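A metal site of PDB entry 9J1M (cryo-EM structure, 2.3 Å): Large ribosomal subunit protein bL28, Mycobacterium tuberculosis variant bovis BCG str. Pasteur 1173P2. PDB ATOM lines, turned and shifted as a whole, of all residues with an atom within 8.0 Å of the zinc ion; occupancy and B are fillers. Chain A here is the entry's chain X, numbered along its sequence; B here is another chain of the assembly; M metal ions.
The backbone carbonyl oxygen of Cys 55 is in hydrogen-bond range of the backbone NH of Lys 60.
The side-chain sulfur (SG) of Cys 52 lies close to the backbone NH (N) of Ser 54 (3.7 Å).
N of Cys 5 lies within hydrogen-bond range of O of Lys 10, 2.9 Å away.
The backbone NH (N) of Lys 10 sits close to the side-chain sulfur (SG) of Cys 8 (3.7 Å).
The side-chain sulfur (SG) of Cys 5 lies close to the backbone NH (N) of Ile 7 (3.4 Å).
Of the 21 residues printed, 4 come within 4 Å of the zinc ion.
SG of Cys 8 is bound to the zinc ion, 2.3 Å away.
SG of Cys 52 binds the zinc ion, at 2.3 Å.
SG of Cys 55 binds the zinc ion (2.3 Å).
SG of Cys 5 is bound to the zinc ion (2.3 Å).
The zinc ion has four donor atoms within binding distance.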
ATOM      1  N   VAL A   4      13.396   0.583   3.696  1.00  0.00           N
ATOM      2  CA  VAL A   4      13.410  -0.878   3.611  1.00  0.00           C
ATOM      3  C   VAL A   4      11.994  -1.376   3.867  1.00  0.00           C
ATOM      4  O   VAL A   4      11.342  -0.933   4.824  1.00  0.00           O
ATOM      5  CB  VAL A   4      14.401  -1.499   4.615  1.00  0.00           C
ATOM      6  CG1 VAL A   4      14.337  -3.011   4.546  1.00  0.00           C
ATOM      7  CG2 VAL A   4      15.807  -1.008   4.352  1.00  0.00           C
ATOM      8  N   CYS A   5      11.517  -2.271   3.008  1.00  0.00           N
ATOM      9  CA  CYS A   5      10.210  -2.873   3.201  1.00  0.00           C
ATOM     10  C   CYS A   5      10.291  -4.017   4.203  1.00  0.00           C
ATOM     11  O   CYS A   5      11.218  -4.830   4.155  1.00  0.00           O
ATOM     12  CB  CYS A   5       9.650  -3.373   1.864  1.00  0.00           C
ATOM     13  SG  CYS A   5       7.984  -4.080   1.941  1.00  0.00           S
ATOM     14  N   ASP A   6       9.307  -4.095   5.105  1.00  0.00           N
ATOM     15  CA  ASP A   6       9.281  -5.184   6.068  1.00  0.00           C
ATOM     16  C   ASP A   6       8.738  -6.486   5.502  1.00  0.00           C
ATOM     17  O   ASP A   6       8.872  -7.525   6.161  1.00  0.00           O
ATOM     18  CB  ASP A   6       8.470  -4.807   7.309  1.00  0.00           C
ATOM     19  CG  ASP A   6       8.991  -3.568   7.991  1.00  0.00           C
ATOM     20  OD1 ASP A   6      10.188  -3.274   7.853  1.00  0.00           O
ATOM     21  OD2 ASP A   6       8.199  -2.915   8.707  1.00  0.00           O
ATOM     22  N   ILE A   7       8.113  -6.480   4.321  1.00  0.00           N
ATOM     23  CA  ILE A   7       7.615  -7.716   3.746  1.00  0.00           C
ATOM     24  C   ILE A   7       8.632  -8.295   2.784  1.00  0.00           C
ATOM     25  O   ILE A   7       9.195  -9.365   3.031  1.00  0.00           O
ATOM     26  CB  ILE A   7       6.254  -7.516   3.034  1.00  0.00           C
ATOM     27  CG1 ILE A   7       5.468  -6.377   3.678  1.00  0.00           C
ATOM     28  CG2 ILE A   7       5.466  -8.807   3.025  1.00  0.00           C
ATOM     29  CD1 ILE A   7       4.981  -6.696   5.067  1.00  0.00           C
ATOM     30  N   CYS A   8       8.907  -7.581   1.699  1.00  0.00           N
ATOM     31  CA  CYS A   8       9.785  -8.094   0.663  1.00  0.00           C
ATOM     32  C   CYS A   8      11.238  -7.686   0.851  1.00  0.00           C
ATOM     33  O   CYS A   8      12.084  -8.075   0.051  1.00  0.00           O
ATOM     34  CB  CYS A   8       9.307  -7.640  -0.719  1.00  0.00           C
ATOM     35  SG  CYS A   8       9.349  -5.866  -1.001  1.00  0.00           S
ATOM     36  N   GLY A   9      11.544  -6.920   1.888  1.00  0.00           N
ATOM     37  CA  GLY A   9      12.915  -6.521   2.137  1.00  0.00           C
ATOM     38  C   GLY A   9      13.523  -5.624   1.088  1.00  0.00           C
ATOM     39  O   GLY A   9      14.742  -5.445   1.077  1.00  0.00           O
ATOM     40  N   LYS A  10      12.709  -5.070   0.193  1.00  0.00           N
ATOM     41  CA  LYS A  10      13.214  -4.177  -0.830  1.00  0.00           C
ATOM     42  C   LYS A  10      13.861  -2.969  -0.193  1.00  0.00           C
ATOM     43  O   LYS A  10      13.292  -2.349   0.711  1.00  0.00           O
ATOM     44  CB  LYS A  10      12.078  -3.767  -1.761  1.00  0.00           C
ATOM     45  CG  LYS A  10      12.473  -2.862  -2.902  1.00  0.00           C
ATOM     46  CD  LYS A  10      11.454  -2.933  -4.030  1.00  0.00           C
ATOM     47  CE  LYS A  10      10.172  -2.205  -3.688  1.00  0.00           C
ATOM     48  NZ  LYS A  10       9.261  -2.209  -4.856  1.00  0.00           N
ATOM     49  N   GLY A  11      15.072  -2.635  -0.643  1.00  0.00           N
ATOM     50  CA  GLY A  11      15.818  -1.539  -0.089  1.00  0.00           C
ATOM     51  C   GLY A  11      16.173  -0.515  -1.142  1.00  0.00           C
ATOM     52  O   GLY A  11      15.756  -0.612  -2.298  1.00  0.00           O
ATOM     53  N   PRO A  31      12.930   2.894  -2.117  1.00  0.00           N
ATOM     54  CA  PRO A  31      11.603   2.368  -2.416  1.00  0.00           C
ATOM     55  C   PRO A  31      10.524   3.258  -1.824  1.00  0.00           C
ATOM     56  O   PRO A  31      10.733   3.933  -0.807  1.00  0.00           O
ATOM     57  CB  PRO A  31      11.611   0.987  -1.769  1.00  0.00           C
ATOM     58  CG  PRO A  31      12.610   1.079  -0.714  1.00  0.00           C
ATOM     59  CD  PRO A  31      13.675   2.007  -1.214  1.00  0.00           C
ATOM     60  N   ASN A  32       9.367   3.260  -2.477  1.00  0.00           N
ATOM     61  CA  ASN A  32       8.229   4.049  -2.013  1.00  0.00           C
ATOM     62  C   ASN A  32       7.641   3.354  -0.797  1.00  0.00           C
ATOM     63  O   ASN A  32       6.668   2.607  -0.863  1.00  0.00           O
ATOM     64  CB  ASN A  32       7.204   4.205  -3.125  1.00  0.00           C
ATOM     65  CG  ASN A  32       6.200   5.297  -2.837  1.00  0.00           C
ATOM     66  OD1 ASN A  32       6.255   5.925  -1.787  1.00  0.00           O
ATOM     67  ND2 ASN A  32       5.295   5.533  -3.770  1.00  0.00           N
ATOM     68  N   ILE A  33       8.265   3.599   0.347  1.00  0.00           N
ATOM     69  CA  ILE A  33       7.904   2.958   1.591  1.00  0.00           C
ATOM     70  C   ILE A  33       6.832   3.781   2.284  1.00  0.00           C
ATOM     71  O   ILE A  33       6.968   4.993   2.435  1.00  0.00           O
ATOM     72  CB  ILE A  33       9.139   2.777   2.498  1.00  0.00           C
ATOM     73  CG1 ILE A  33      10.154   1.881   1.809  1.00  0.00           C
ATOM     74  CG2 ILE A  33       8.734   2.213   3.834  1.00  0.00           C
ATOM     75  CD1 ILE A  33       9.749   0.441   1.759  1.00  0.00           C
ATOM     76  N   ASN A  50       6.344  -0.562   7.868  1.00  0.00           N
ATOM     77  CA  ASN A  50       6.618   0.300   6.729  1.00  0.00           C
ATOM     78  C   ASN A  50       6.898  -0.603   5.535  1.00  0.00           C
ATOM     79  O   ASN A  50       7.867  -1.373   5.531  1.00  0.00           O
ATOM     80  CB  ASN A  50       7.742   1.297   7.024  1.00  0.00           C
ATOM     81  CG  ASN A  50       8.867   0.708   7.826  1.00  0.00           C
ATOM     82  OD1 ASN A  50       9.362   1.307   8.776  1.00  0.00           O
ATOM     83  ND2 ASN A  50       9.300  -0.479   7.429  1.00  0.00           N
ATOM     84  N   VAL A  51       6.014  -0.561   4.553  1.00  0.00           N
ATOM     85  CA  VAL A  51       6.041  -1.470   3.426  1.00  0.00           C
ATOM     86  C   VAL A  51       5.996  -0.647   2.141  1.00  0.00           C
ATOM     87  O   VAL A  51       5.562   0.507   2.136  1.00  0.00           O
ATOM     88  CB  VAL A  51       4.875  -2.480   3.462  1.00  0.00           C
ATOM     89  CG1 VAL A  51       4.782  -3.128   4.832  1.00  0.00           C
ATOM     90  CG2 VAL A  51       3.575  -1.816   3.114  1.00  0.00           C
ATOM     91  N   CYS A  52       6.465  -1.254   1.068  1.00  0.00           N
ATOM     92  CA  CYS A  52       6.487  -0.538  -0.200  1.00  0.00           C
ATOM     93  C   CYS A  52       5.099  -0.514  -0.826  1.00  0.00           C
ATOM     94  O   CYS A  52       4.233  -1.354  -0.557  1.00  0.00           O
ATOM     95  CB  CYS A  52       7.500  -1.159  -1.156  1.00  0.00           C
ATOM     96  SG  CYS A  52       7.120  -2.832  -1.692  1.00  0.00           S
ATOM     97  N   THR A  53       4.882   0.493  -1.670  1.00  0.00           N
ATOM     98  CA  THR A  53       3.626   0.597  -2.396  1.00  0.00           C
ATOM     99  C   THR A  53       3.394  -0.596  -3.307  1.00  0.00           C
ATOM    100  O   THR A  53       2.249  -0.880  -3.650  1.00  0.00           O
ATOM    101  CB  THR A  53       3.590   1.879  -3.215  1.00  0.00           C
ATOM    102  OG1 THR A  53       4.781   1.988  -3.994  1.00  0.00           O
ATOM    103  CG2 THR A  53       3.454   3.086  -2.305  1.00  0.00           C
ATOM    104  N   SER A  54       4.451  -1.307  -3.714  1.00  0.00           N
ATOM    105  CA  SER A  54       4.244  -2.526  -4.488  1.00  0.00           C
ATOM    106  C   SER A  54       3.531  -3.593  -3.657  1.00  0.00           C
ATOM    107  O   SER A  54       2.590  -4.233  -4.130  1.00  0.00           O
ATOM    108  CB  SER A  54       5.576  -3.068  -5.003  1.00  0.00           C
ATOM    109  OG  SER A  54       6.172  -2.157  -5.911  1.00  0.00           O
ATOM    110  N   CYS A  55       3.957  -3.775  -2.399  1.00  0.00           N
ATOM    111  CA  CYS A  55       3.270  -4.715  -1.527  1.00  0.00           C
ATOM    112  C   CYS A  55       1.891  -4.214  -1.148  1.00  0.00           C
ATOM    113  O   CYS A  55       0.987  -5.020  -0.918  1.00  0.00           O
ATOM    114  CB  CYS A  55       4.104  -4.974  -0.268  1.00  0.00           C
ATOM    115  SG  CYS A  55       5.615  -5.929  -0.527  1.00  0.00           S
ATOM    116  N   ILE A  56       1.696  -2.892  -1.061  1.00  0.00           N
ATOM    117  CA  ILE A  56       0.355  -2.379  -0.784  1.00  0.00           C
ATOM    118  C   ILE A  56      -0.571  -2.622  -1.966  1.00  0.00           C
ATOM    119  O   ILE A  56      -1.734  -2.994  -1.799  1.00  0.00           O
ATOM    120  CB  ILE A  56       0.413  -0.888  -0.407  1.00  0.00           C
ATOM    121  CG1 ILE A  56       0.872  -0.704   1.043  1.00  0.00           C
ATOM    122  CG2 ILE A  56      -0.958  -0.251  -0.542  1.00  0.00           C
ATOM    123  CD1 ILE A  56       1.537   0.631   1.280  1.00  0.00           C
ATOM    124  N   LYS A  60      -0.485  -8.037  -0.027  1.00  0.00           N
ATOM    125  CA  LYS A  60       0.452  -8.521   0.984  1.00  0.00           C
ATOM    126  C   LYS A  60       0.118  -8.032   2.386  1.00  0.00           C
ATOM    127  O   LYS A  60       0.511  -8.669   3.358  1.00  0.00           O
ATOM    128  CB  LYS A  60       1.873  -8.117   0.625  1.00  0.00           C
ATOM    129  CG  LYS A  60       2.203  -8.313  -0.840  1.00  0.00           C
ATOM    130  CD  LYS A  60       2.384  -9.775  -1.180  1.00  0.00           C
ATOM    131  CE  LYS A  60       3.843 -10.113  -1.404  1.00  0.00           C
ATOM    132  NZ  LYS A  60       4.251  -9.883  -2.815  1.00  0.00           N
ATOM    133  N   ILE A  61      -0.596  -6.908   2.509  1.00  0.00           N
ATOM    134  CA  ILE A  61      -0.968  -6.371   3.807  1.00  0.00           C
ATOM    135  C   ILE A  61      -2.453  -6.060   3.821  1.00  0.00           C
ATOM    136  O   ILE A  61      -3.097  -5.870   2.783  1.00  0.00           O
ATOM    137  CB  ILE A  61      -0.109  -5.148   4.206  1.00  0.00           C
ATOM    138  CG1 ILE A  61      -0.118  -4.021   3.162  1.00  0.00           C
ATOM    139  CG2 ILE A  61       1.321  -5.567   4.521  1.00  0.00           C
ATOM    140  CD1 ILE A  61      -1.409  -3.210   3.017  1.00  0.00           C
ATOM    141  P     U B 486      10.141   1.098  -5.623  1.00  0.00           P
ATOM    142  OP1   U B 486       9.409   1.156  -4.340  1.00  0.00           O
ATOM    143  OP2   U B 486      10.031  -0.100  -6.482  1.00  0.00           O
ATOM    144  O5'   U B 486       9.670   2.329  -6.498  1.00  0.00           O
ATOM    145  C5'   U B 486       9.678   3.650  -5.984  1.00  0.00           C
ATOM    146  C4'   U B 486       9.108   4.609  -6.987  1.00  0.00           C
ATOM    147  O4'   U B 486      10.014   4.749  -8.108  1.00  0.00           O
ATOM    148  C3'   U B 486       7.811   4.155  -7.631  1.00  0.00           C
ATOM    149  O3'   U B 486       6.677   4.389  -6.831  1.00  0.00           O
ATOM    150  C2'   U B 486       7.810   4.921  -8.947  1.00  0.00           C
ATOM    151  O2'   U B 486       7.423   6.269  -8.756  1.00  0.00           O
ATOM    152  C1'   U B 486       9.287   4.888  -9.307  1.00  0.00           C
ATOM    153  N1    U B 486       9.607   3.743 -10.189  1.00  0.00           N
ATOM    154  C2    U B 486       9.357   3.900 -11.523  1.00  0.00           C
ATOM    155  O2    U B 486       8.895   4.927 -11.990  1.00  0.00           O
ATOM    156  N3    U B 486       9.670   2.827 -12.307  1.00  0.00           N
ATOM    157  C4    U B 486      10.188   1.634 -11.887  1.00  0.00           C
ATOM    158  O4    U B 486      10.413   0.742 -12.702  1.00  0.00           O
ATOM    159  C5    U B 486      10.413   1.544 -10.481  1.00  0.00           C
ATOM    160  C6    U B 486      10.131   2.581  -9.695  1.00  0.00           C
HETATM  161 ZN    ZN M   1       7.526  -4.625  -0.278  1.00  0.00          ZN
